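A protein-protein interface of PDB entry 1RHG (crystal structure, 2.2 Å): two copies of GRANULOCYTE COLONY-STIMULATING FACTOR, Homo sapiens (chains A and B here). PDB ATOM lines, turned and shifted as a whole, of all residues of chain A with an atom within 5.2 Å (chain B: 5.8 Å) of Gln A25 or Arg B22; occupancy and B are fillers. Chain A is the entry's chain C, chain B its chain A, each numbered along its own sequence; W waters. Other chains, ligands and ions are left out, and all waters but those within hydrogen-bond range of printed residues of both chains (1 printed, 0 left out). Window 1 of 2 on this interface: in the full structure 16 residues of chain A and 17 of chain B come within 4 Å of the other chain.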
ATOM      1  N   GLN A  20      11.893  11.920  19.376  1.00  0.00           N
ATOM      2  CA  GLN A  20      13.209  11.442  19.780  1.00  0.00           C
ATOM      3  C   GLN A  20      14.301  12.057  18.909  1.00  0.00           C
ATOM      4  O   GLN A  20      15.358  12.389  19.455  1.00  0.00           O
ATOM      5  CB  GLN A  20      13.301   9.926  19.689  1.00  0.00           C
ATOM      6  CG  GLN A  20      12.679   9.180  20.855  1.00  0.00           C
ATOM      7  CD  GLN A  20      12.636   7.668  20.608  1.00  0.00           C
ATOM      8  OE1 GLN A  20      12.407   7.230  19.481  1.00  0.00           O
ATOM      9  NE2 GLN A  20      12.853   6.746  21.544  1.00  0.00           N
ATOM     10  N   VAL A  21      14.137  12.326  17.618  1.00  0.00           N
ATOM     11  CA  VAL A  21      15.140  13.062  16.877  1.00  0.00           C
ATOM     12  C   VAL A  21      15.411  14.379  17.607  1.00  0.00           C
ATOM     13  O   VAL A  21      16.540  14.638  18.029  1.00  0.00           O
ATOM     14  CB  VAL A  21      14.612  13.330  15.466  1.00  0.00           C
ATOM     15  CG1 VAL A  21      15.470  14.291  14.693  1.00  0.00           C
ATOM     16  CG2 VAL A  21      14.602  12.006  14.737  1.00  0.00           C
ATOM     17  N   ARG A  22      14.376  15.177  17.941  1.00  0.00           N
ATOM     18  CA  ARG A  22      14.572  16.494  18.543  1.00  0.00           C
ATOM     19  C   ARG A  22      15.175  16.333  19.893  1.00  0.00           C
ATOM     20  O   ARG A  22      16.076  17.076  20.206  1.00  0.00           O
ATOM     21  CB  ARG A  22      13.281  17.289  18.701  1.00  0.00           C
ATOM     22  CG  ARG A  22      12.575  17.636  17.405  1.00  0.00           C
ATOM     23  CD  ARG A  22      13.489  18.180  16.317  1.00  0.00           C
ATOM     24  NE  ARG A  22      12.724  18.657  15.180  1.00  0.00           N
ATOM     25  CZ  ARG A  22      13.247  18.971  13.994  1.00  0.00           C
ATOM     26  NH1 ARG A  22      14.536  18.880  13.657  1.00  0.00           N
ATOM     27  NH2 ARG A  22      12.426  19.541  13.125  1.00  0.00           N
ATOM     28  N   LYS A  23      14.831  15.361  20.689  1.00  0.00           N
ATOM     29  CA  LYS A  23      15.415  15.223  22.009  1.00  0.00           C
ATOM     30  C   LYS A  23      16.887  14.907  21.842  1.00  0.00           C
ATOM     31  O   LYS A  23      17.671  15.267  22.719  1.00  0.00           O
ATOM     32  CB  LYS A  23      14.744  14.103  22.747  1.00  0.00           C
ATOM     33  CG  LYS A  23      15.054  14.131  24.211  1.00  0.00           C
ATOM     34  CD  LYS A  23      14.573  12.816  24.831  1.00  0.00           C
ATOM     35  CE  LYS A  23      13.067  12.487  24.711  1.00  0.00           C
ATOM     36  NZ  LYS A  23      12.840  11.065  24.943  1.00  0.00           N
ATOM     37  N   ILE A  24      17.364  14.289  20.759  1.00  0.00           N
ATOM     38  CA  ILE A  24      18.801  14.033  20.653  1.00  0.00           C
ATOM     39  C   ILE A  24      19.448  15.306  20.144  1.00  0.00           C
ATOM     40  O   ILE A  24      20.553  15.637  20.577  1.00  0.00           O
ATOM     41  CB  ILE A  24      19.073  12.817  19.677  1.00  0.00           C
ATOM     42  CG1 ILE A  24      18.464  11.611  20.337  1.00  0.00           C
ATOM     43  CG2 ILE A  24      20.540  12.528  19.429  1.00  0.00           C
ATOM     44  CD1 ILE A  24      18.146  10.495  19.315  1.00  0.00           C
ATOM     45  N   GLN A  25      18.821  16.052  19.234  1.00  0.00           N
ATOM     46  CA  GLN A  25      19.396  17.292  18.713  1.00  0.00           C
ATOM     47  C   GLN A  25      19.580  18.283  19.844  1.00  0.00           C
ATOM     48  O   GLN A  25      20.554  19.041  19.878  1.00  0.00           O
ATOM     49  CB  GLN A  25      18.515  17.946  17.683  1.00  0.00           C
ATOM     50  CG  GLN A  25      18.434  17.053  16.497  1.00  0.00           C
ATOM     51  CD  GLN A  25      17.692  17.546  15.290  1.00  0.00           C
ATOM     52  OE1 GLN A  25      16.487  17.661  15.279  1.00  0.00           O
ATOM     53  NE2 GLN A  25      18.276  17.708  14.129  1.00  0.00           N
ATOM     54  N   GLY A  26      18.675  18.287  20.824  1.00  0.00           N
ATOM     55  CA  GLY A  26      18.835  19.093  22.002  1.00  0.00           C
ATOM     56  C   GLY A  26      20.111  18.724  22.752  1.00  0.00           C
ATOM     57  O   GLY A  26      20.949  19.606  22.923  1.00  0.00           O
ATOM     58  N   ASP A  27      20.286  17.464  23.186  1.00  0.00           N
ATOM     59  CA  ASP A  27      21.494  17.061  23.886  1.00  0.00           C
ATOM     60  C   ASP A  27      22.754  17.350  23.076  1.00  0.00           C
ATOM     61  O   ASP A  27      23.749  17.800  23.625  1.00  0.00           O
ATOM     62  CB  ASP A  27      21.544  15.610  24.170  1.00  0.00           C
ATOM     63  CG  ASP A  27      20.285  14.933  24.629  1.00  0.00           C
ATOM     64  OD1 ASP A  27      19.574  15.398  25.502  1.00  0.00           O
ATOM     65  OD2 ASP A  27      20.031  13.876  24.104  1.00  0.00           O
ATOM     66  N   GLY A  28      22.692  17.197  21.767  1.00  0.00           N
ATOM     67  CA  GLY A  28      23.812  17.433  20.925  1.00  0.00           C
ATOM     68  C   GLY A  28      24.203  18.884  21.035  1.00  0.00           C
ATOM     69  O   GLY A  28      25.325  19.184  21.457  1.00  0.00           O
ATOM     70  N   ALA A  29      23.267  19.794  20.720  1.00  0.00           N
ATOM     71  CA  ALA A  29      23.474  21.238  20.784  1.00  0.00           C
ATOM     72  C   ALA A  29      23.897  21.626  22.192  1.00  0.00           C
ATOM     73  O   ALA A  29      24.633  22.585  22.341  1.00  0.00           O
ATOM     74  CB  ALA A  29      22.186  21.975  20.474  1.00  0.00           C
ATOM     75  N   ALA A  30      23.517  20.898  23.233  1.00  0.00           N
ATOM     76  CA  ALA A  30      23.928  21.226  24.561  1.00  0.00           C
ATOM     77  C   ALA A  30      25.377  20.867  24.720  1.00  0.00           C
ATOM     78  O   ALA A  30      26.128  21.674  25.269  1.00  0.00           O
ATOM     79  CB  ALA A  30      23.149  20.448  25.602  1.00  0.00           C
ATOM     80  N   GLN A 158      24.116  15.862  14.699  1.00  0.00           N
ATOM     81  CA  GLN A 158      23.105  16.889  14.457  1.00  0.00           C
ATOM     82  C   GLN A 158      22.526  16.874  13.028  1.00  0.00           C
ATOM     83  O   GLN A 158      21.295  16.762  12.834  1.00  0.00           O
ATOM     84  CB  GLN A 158      23.745  18.246  14.791  1.00  0.00           C
ATOM     85  CG  GLN A 158      22.831  19.475  14.865  1.00  0.00           C
ATOM     86  CD  GLN A 158      21.726  19.508  15.931  1.00  0.00           C
ATOM     87  OE1 GLN A 158      20.628  20.026  15.681  1.00  0.00           O
ATOM     88  NE2 GLN A 158      21.911  18.964  17.116  1.00  0.00           N
ATOM     89  N   LEU A 161      20.766  13.647  11.998  1.00  0.00           N
ATOM     90  CA  LEU A 161      19.438  13.589  12.542  1.00  0.00           C
ATOM     91  C   LEU A 161      18.563  14.512  11.797  1.00  0.00           C
ATOM     92  O   LEU A 161      17.377  14.208  11.696  1.00  0.00           O
ATOM     93  CB  LEU A 161      19.441  13.968  13.968  1.00  0.00           C
ATOM     94  CG  LEU A 161      19.823  12.841  14.863  1.00  0.00           C
ATOM     95  CD1 LEU A 161      20.114  13.376  16.194  1.00  0.00           C
ATOM     96  CD2 LEU A 161      18.733  11.817  14.934  1.00  0.00           C
ATOM     97  N   GLU A 162      19.070  15.594  11.240  1.00  0.00           N
ATOM     98  CA  GLU A 162      18.154  16.436  10.531  1.00  0.00           C
ATOM     99  C   GLU A 162      17.664  15.660   9.323  1.00  0.00           C
ATOM    100  O   GLU A 162      16.465  15.467   9.156  1.00  0.00           O
ATOM    101  CB  GLU A 162      18.825  17.710  10.081  1.00  0.00           C
ATOM    102  CG  GLU A 162      19.274  18.526  11.251  1.00  0.00           C
ATOM    103  CD  GLU A 162      20.473  19.424  10.969  1.00  0.00           C
ATOM    104  OE1 GLU A 162      20.741  19.713   9.781  1.00  0.00           O
ATOM    105  OE2 GLU A 162      21.140  19.811  11.954  1.00  0.00           O
ATOM    106  N   CYS B  17      20.924  29.505  21.389  1.00  0.00           N
ATOM    107  CA  CYS B  17      19.742  29.516  20.569  1.00  0.00           C
ATOM    108  C   CYS B  17      19.500  28.122  19.994  1.00  0.00           C
ATOM    109  O   CYS B  17      18.372  27.644  20.216  1.00  0.00           O
ATOM    110  CB  CYS B  17      19.865  30.439  19.422  1.00  0.00           C
ATOM    111  SG  CYS B  17      20.009  32.129  20.017  1.00  0.00           S
ATOM    112  N   LEU B  18      20.434  27.381  19.335  1.00  0.00           N
ATOM    113  CA  LEU B  18      20.125  26.047  18.791  1.00  0.00           C
ATOM    114  C   LEU B  18      19.538  25.074  19.797  1.00  0.00           C
ATOM    115  O   LEU B  18      18.546  24.402  19.513  1.00  0.00           O
ATOM    116  CB  LEU B  18      21.369  25.359  18.151  1.00  0.00           C
ATOM    117  CG  LEU B  18      21.167  23.921  17.545  1.00  0.00           C
ATOM    118  CD1 LEU B  18      20.229  23.949  16.365  1.00  0.00           C
ATOM    119  CD2 LEU B  18      22.482  23.382  16.964  1.00  0.00           C
ATOM    120  N   GLU B  19      20.093  25.006  20.981  1.00  0.00           N
ATOM    121  CA  GLU B  19      19.534  24.195  22.048  1.00  0.00           C
ATOM    122  C   GLU B  19      18.090  24.600  22.473  1.00  0.00           C
ATOM    123  O   GLU B  19      17.251  23.776  22.897  1.00  0.00           O
ATOM    124  CB  GLU B  19      20.557  24.366  23.097  1.00  0.00           C
ATOM    125  CG  GLU B  19      20.458  23.980  24.551  1.00  0.00           C
ATOM    126  CD  GLU B  19      21.787  24.337  25.266  1.00  0.00           C
ATOM    127  OE1 GLU B  19      22.613  25.151  24.796  1.00  0.00           O
ATOM    128  OE2 GLU B  19      22.020  23.760  26.329  1.00  0.00           O
ATOM    129  N   GLN B  20      17.757  25.894  22.347  1.00  0.00           N
ATOM    130  CA  GLN B  20      16.453  26.413  22.732  1.00  0.00           C
ATOM    131  C   GLN B  20      15.479  26.084  21.637  1.00  0.00           C
ATOM    132  O   GLN B  20      14.417  25.535  21.915  1.00  0.00           O
ATOM    133  CB  GLN B  20      16.580  27.923  22.995  1.00  0.00           C
ATOM    134  CG  GLN B  20      17.079  28.003  24.451  1.00  0.00           C
ATOM    135  CD  GLN B  20      17.240  29.383  25.080  1.00  0.00           C
ATOM    136  OE1 GLN B  20      16.762  29.634  26.198  1.00  0.00           O
ATOM    137  NE2 GLN B  20      17.898  30.340  24.424  1.00  0.00           N
ATOM    138  N   VAL B  21      15.900  26.323  20.400  1.00  0.00           N
ATOM    139  CA  VAL B  21      15.174  25.930  19.210  1.00  0.00           C
ATOM    140  C   VAL B  21      14.896  24.419  19.318  1.00  0.00           C
ATOM    141  O   VAL B  21      13.693  24.065  19.325  1.00  0.00           O
ATOM    142  CB  VAL B  21      16.021  26.268  17.976  1.00  0.00           C
ATOM    143  CG1 VAL B  21      15.404  25.666  16.763  1.00  0.00           C
ATOM    144  CG2 VAL B  21      16.079  27.749  17.753  1.00  0.00           C
ATOM    145  N   ARG B  22      15.863  23.483  19.517  1.00  0.00           N
ATOM    146  CA  ARG B  22      15.551  22.037  19.575  1.00  0.00           C
ATOM    147  C   ARG B  22      14.653  21.673  20.741  1.00  0.00           C
ATOM    148  O   ARG B  22      13.838  20.739  20.685  1.00  0.00           O
ATOM    149  CB  ARG B  22      16.844  21.198  19.659  1.00  0.00           C
ATOM    150  CG  ARG B  22      17.825  21.456  18.523  1.00  0.00           C
ATOM    151  CD  ARG B  22      17.087  21.311  17.215  1.00  0.00           C
ATOM    152  NE  ARG B  22      18.006  21.191  16.101  1.00  0.00           N
ATOM    153  CZ  ARG B  22      17.634  21.426  14.841  1.00  0.00           C
ATOM    154  NH1 ARG B  22      16.348  21.784  14.642  1.00  0.00           N
ATOM    155  NH2 ARG B  22      18.528  21.338  13.805  1.00  0.00           N
ATOM    156  N   LYS B  23      14.721  22.482  21.801  1.00  0.00           N
ATOM    157  CA  LYS B  23      13.919  22.242  23.010  1.00  0.00           C
ATOM    158  C   LYS B  23      12.444  22.493  22.743  1.00  0.00           C
ATOM    159  O   LYS B  23      11.574  21.676  23.061  1.00  0.00           O
ATOM    160  CB  LYS B  23      14.389  23.167  24.114  1.00  0.00           C
ATOM    161  CG  LYS B  23      13.817  22.669  25.432  1.00  0.00           C
ATOM    162  CD  LYS B  23      14.159  23.552  26.592  1.00  0.00           C
ATOM    163  CE  LYS B  23      15.655  23.563  26.867  1.00  0.00           C
ATOM    164  NZ  LYS B  23      15.983  24.732  27.680  1.00  0.00           N
ATOM    165  N   ILE B  24      12.132  23.619  22.106  1.00  0.00           N
ATOM    166  CA  ILE B  24      10.751  23.958  21.804  1.00  0.00           C
ATOM    167  C   ILE B  24      10.250  22.961  20.771  1.00  0.00           C
ATOM    168  O   ILE B  24       9.126  22.453  20.974  1.00  0.00           O
ATOM    169  CB  ILE B  24      10.638  25.361  21.226  1.00  0.00           C
ATOM    170  CG1 ILE B  24      11.146  26.392  22.203  1.00  0.00           C
ATOM    171  CG2 ILE B  24       9.191  25.630  20.897  1.00  0.00           C
ATOM    172  CD1 ILE B  24      11.848  27.532  21.447  1.00  0.00           C
ATOM    173  N   GLN B  25      11.028  22.658  19.687  1.00  0.00           N
ATOM    174  CA  GLN B  25      10.600  21.652  18.718  1.00  0.00           C
ATOM    175  C   GLN B  25      10.333  20.358  19.437  1.00  0.00           C
ATOM    176  O   GLN B  25       9.287  19.757  19.211  1.00  0.00           O
ATOM    177  CB  GLN B  25      11.619  21.360  17.683  1.00  0.00           C
ATOM    178  CG  GLN B  25      11.821  22.622  16.976  1.00  0.00           C
ATOM    179  CD  GLN B  25      12.756  22.475  15.829  1.00  0.00           C
ATOM    180  OE1 GLN B  25      13.795  21.832  15.931  1.00  0.00           O
ATOM    181  NE2 GLN B  25      12.448  23.099  14.696  1.00  0.00           N
ATOM    182  N   GLY B  26      11.101  19.906  20.398  1.00  0.00           N
ATOM    183  CA  GLY B  26      10.790  18.652  21.057  1.00  0.00           C
ATOM    184  C   GLY B  26       9.487  18.709  21.816  1.00  0.00           C
ATOM    185  O   GLY B  26       8.741  17.733  21.791  1.00  0.00           O
ATOM    186  N   ASP B  27       9.177  19.828  22.480  1.00  0.00           N
ATOM    187  CA  ASP B  27       7.875  20.012  23.145  1.00  0.00           C
ATOM    188  C   ASP B  27       6.745  20.042  22.098  1.00  0.00           C
ATOM    189  O   ASP B  27       5.703  19.467  22.328  1.00  0.00           O
ATOM    190  CB  ASP B  27       7.758  21.327  23.861  1.00  0.00           C
ATOM    191  CG  ASP B  27       8.898  21.835  24.721  1.00  0.00           C
ATOM    192  OD1 ASP B  27       9.426  21.062  25.519  1.00  0.00           O
ATOM    193  OD2 ASP B  27       9.205  23.026  24.603  1.00  0.00           O
ATOM    194  N   GLU B 162      12.305  25.681  12.444  1.00  0.00           N
ATOM    195  CA  GLU B 162      13.383  25.250  11.595  1.00  0.00           C
ATOM    196  C   GLU B 162      13.981  26.372  10.791  1.00  0.00           C
ATOM    197  O   GLU B 162      15.201  26.516  10.753  1.00  0.00           O
ATOM    198  CB  GLU B 162      12.902  24.109  10.684  1.00  0.00           C
ATOM    199  CG  GLU B 162      12.981  22.776  11.439  1.00  0.00           C
ATOM    200  CD  GLU B 162      14.369  22.429  12.028  1.00  0.00           C
ATOM    201  OE1 GLU B 162      14.882  23.113  12.935  1.00  0.00           O
ATOM    202  OE2 GLU B 162      14.944  21.437  11.578  1.00  0.00           O
ATOM    203  N   TYR B 165      16.203  28.402  12.887  1.00  0.00           N
ATOM    204  CA  TYR B 165      17.391  27.577  12.976  1.00  0.00           C
ATOM    205  C   TYR B 165      18.229  27.885  11.725  1.00  0.00           C
ATOM    206  O   TYR B 165      19.410  28.241  11.872  1.00  0.00           O
ATOM    207  CB  TYR B 165      16.942  26.087  13.069  1.00  0.00           C
ATOM    208  CG  TYR B 165      18.009  25.082  12.683  1.00  0.00           C
ATOM    209  CD1 TYR B 165      19.178  24.990  13.411  1.00  0.00           C
ATOM    210  CD2 TYR B 165      17.829  24.318  11.551  1.00  0.00           C
ATOM    211  CE1 TYR B 165      20.177  24.143  13.004  1.00  0.00           C
ATOM    212  CE2 TYR B 165      18.823  23.468  11.130  1.00  0.00           C
ATOM    213  CZ  TYR B 165      19.987  23.393  11.863  1.00  0.00           C
ATOM    214  OH  TYR B 165      21.017  22.582  11.407  1.00  0.00           O
HETATM  215  O   HOH W   1      16.393  19.038  11.253  1.00  0.00           O
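Arg A22 touches its own counterpart, Arg B22.
Arg A22 touches Gln B25, and with the chains exchanged Gln A25 touches Arg B22.
Arg A22 touches Gly B26, and with the chains exchanged Gly A26 touches Arg B22.
Arg A22 touches Glu B162, and with the chains exchanged Glu A162 touches Arg B22.
9 positions are printed for both chains.
Of the 12 pairs that touch across the chains among the printed residues, 7 have their exchanged pair printed and touching as well.
NE of Arg B22 lies within hydrogen-bond range of OE1 of Gln A158, 2.9 Å away.
The side-chain carboxylate (OE2) of Glu A162 lies within salt-bridge range of the guanidinium group (NH2) of Arg B22, at 3.5 Å.
The side-chain amide oxygen (OE1) of Gln B25 sits at hydrogen-bond distance from the guanidinium group (NE) of Arg A22 (3.4 Å).
The side-chain carboxylate (OE2) of Glu B162 is in salt-bridge range of the guanidinium group (NH1) of Arg A22, 3.3 Å away.
The side-chain carboxylate (OE2) of Glu A162 lies within hydrogen-bond range of the side-chain hydroxyl (OH) of Tyr B165 (2.8 Å).
NH1 of Arg B22 sits at hydrogen-bond distance from OE1 of Gln B25, at 2.9 Å.
The guanidinium group of Arg B22 lies within salt-bridge range of the side-chain carboxylate of Glu B162 (2.6 Å).
NE2 of Gln B25 sits at hydrogen-bond distance from OE1 of Glu B162 (3.0 Å).
NH1 of Arg A22 sits at hydrogen-bond distance from OE1 of Gln A25, at 2.8 Å.
The backbone carbonyl oxygen (O) of Gln A25 sits at hydrogen-bond distance from the side-chain amide nitrogen (NE2) of Gln A158 (3.1 Å).
Among the printed residues, pairs that only touch across the chains: Arg A22 with Arg B22 (3.6 Å), Arg A22 with Gly B26 (3.7 Å), Gln A25 with Arg B22 (3.6 Å), Gly A26 with Arg B22 (3.6 Å), Ala A29 with Leu B18 (3.7 Å), Ala A29 with Glu B19 (3.7 Å) and Ala A30 with Glu B19 (3.6 Å).
Of chain B, only Arg B22 (3.6 Å) comes within 4 Å of Gln A25.
Of chain A, only Arg A22 (3.6 Å), Gln A25 (3.6 Å), Gly A26 (3.6 Å), Gln A158 (2.9 Å) and Glu A162 (3.5 Å) come within 4 Å of Arg B22.
Of the printed residues of chain A, Glu B19 touches Ala A29 (3.7 Å) and Ala A30 (3.6 Å).
Of the printed residues of chain B, Gln A158 touches Arg B22 (2.9 Å).
The nearest residue of chain B that does not touch Gln A25 is Gln B25 (5.0 Å).
The nearest printed residue of chain A that does not touch Leu B18 is Gln A158 (4.002 Å).
Water W1 lies within hydrogen-bond range of the side-chain carboxylate (OE2) of Glu B162 and the guanidinium group (NH1) of Arg A22.
Of the 13 printed residues of chain B, 7 touch a printed residue of chain A.
Printed residues of chain B that touch a printed residue of chain A: Leu B18, Glu B19, Arg B22, Gln B25, Gly B26, Glu B162 and Tyr B165.
Hydrophobic or aromatic side chains of chain B within 4 Å of the printed part of chain A: Leu B18 and Tyr B165.
Printed residues of chain A that touch a printed residue of chain B: Arg A22, Gln A25, Gly A26, Ala A29, Ala A30, Gln A158 and Glu A162.
Among the printed residues, 12 pairs touch across the chains.
Among the printed residues, Asp or Glu carboxylates within 4 Å of a Lys or Arg side-chain nitrogen of the other chain: Arg A22 with Glu B162 (3.3 Å) and Glu A162 with Arg B22 (3.5 Å).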
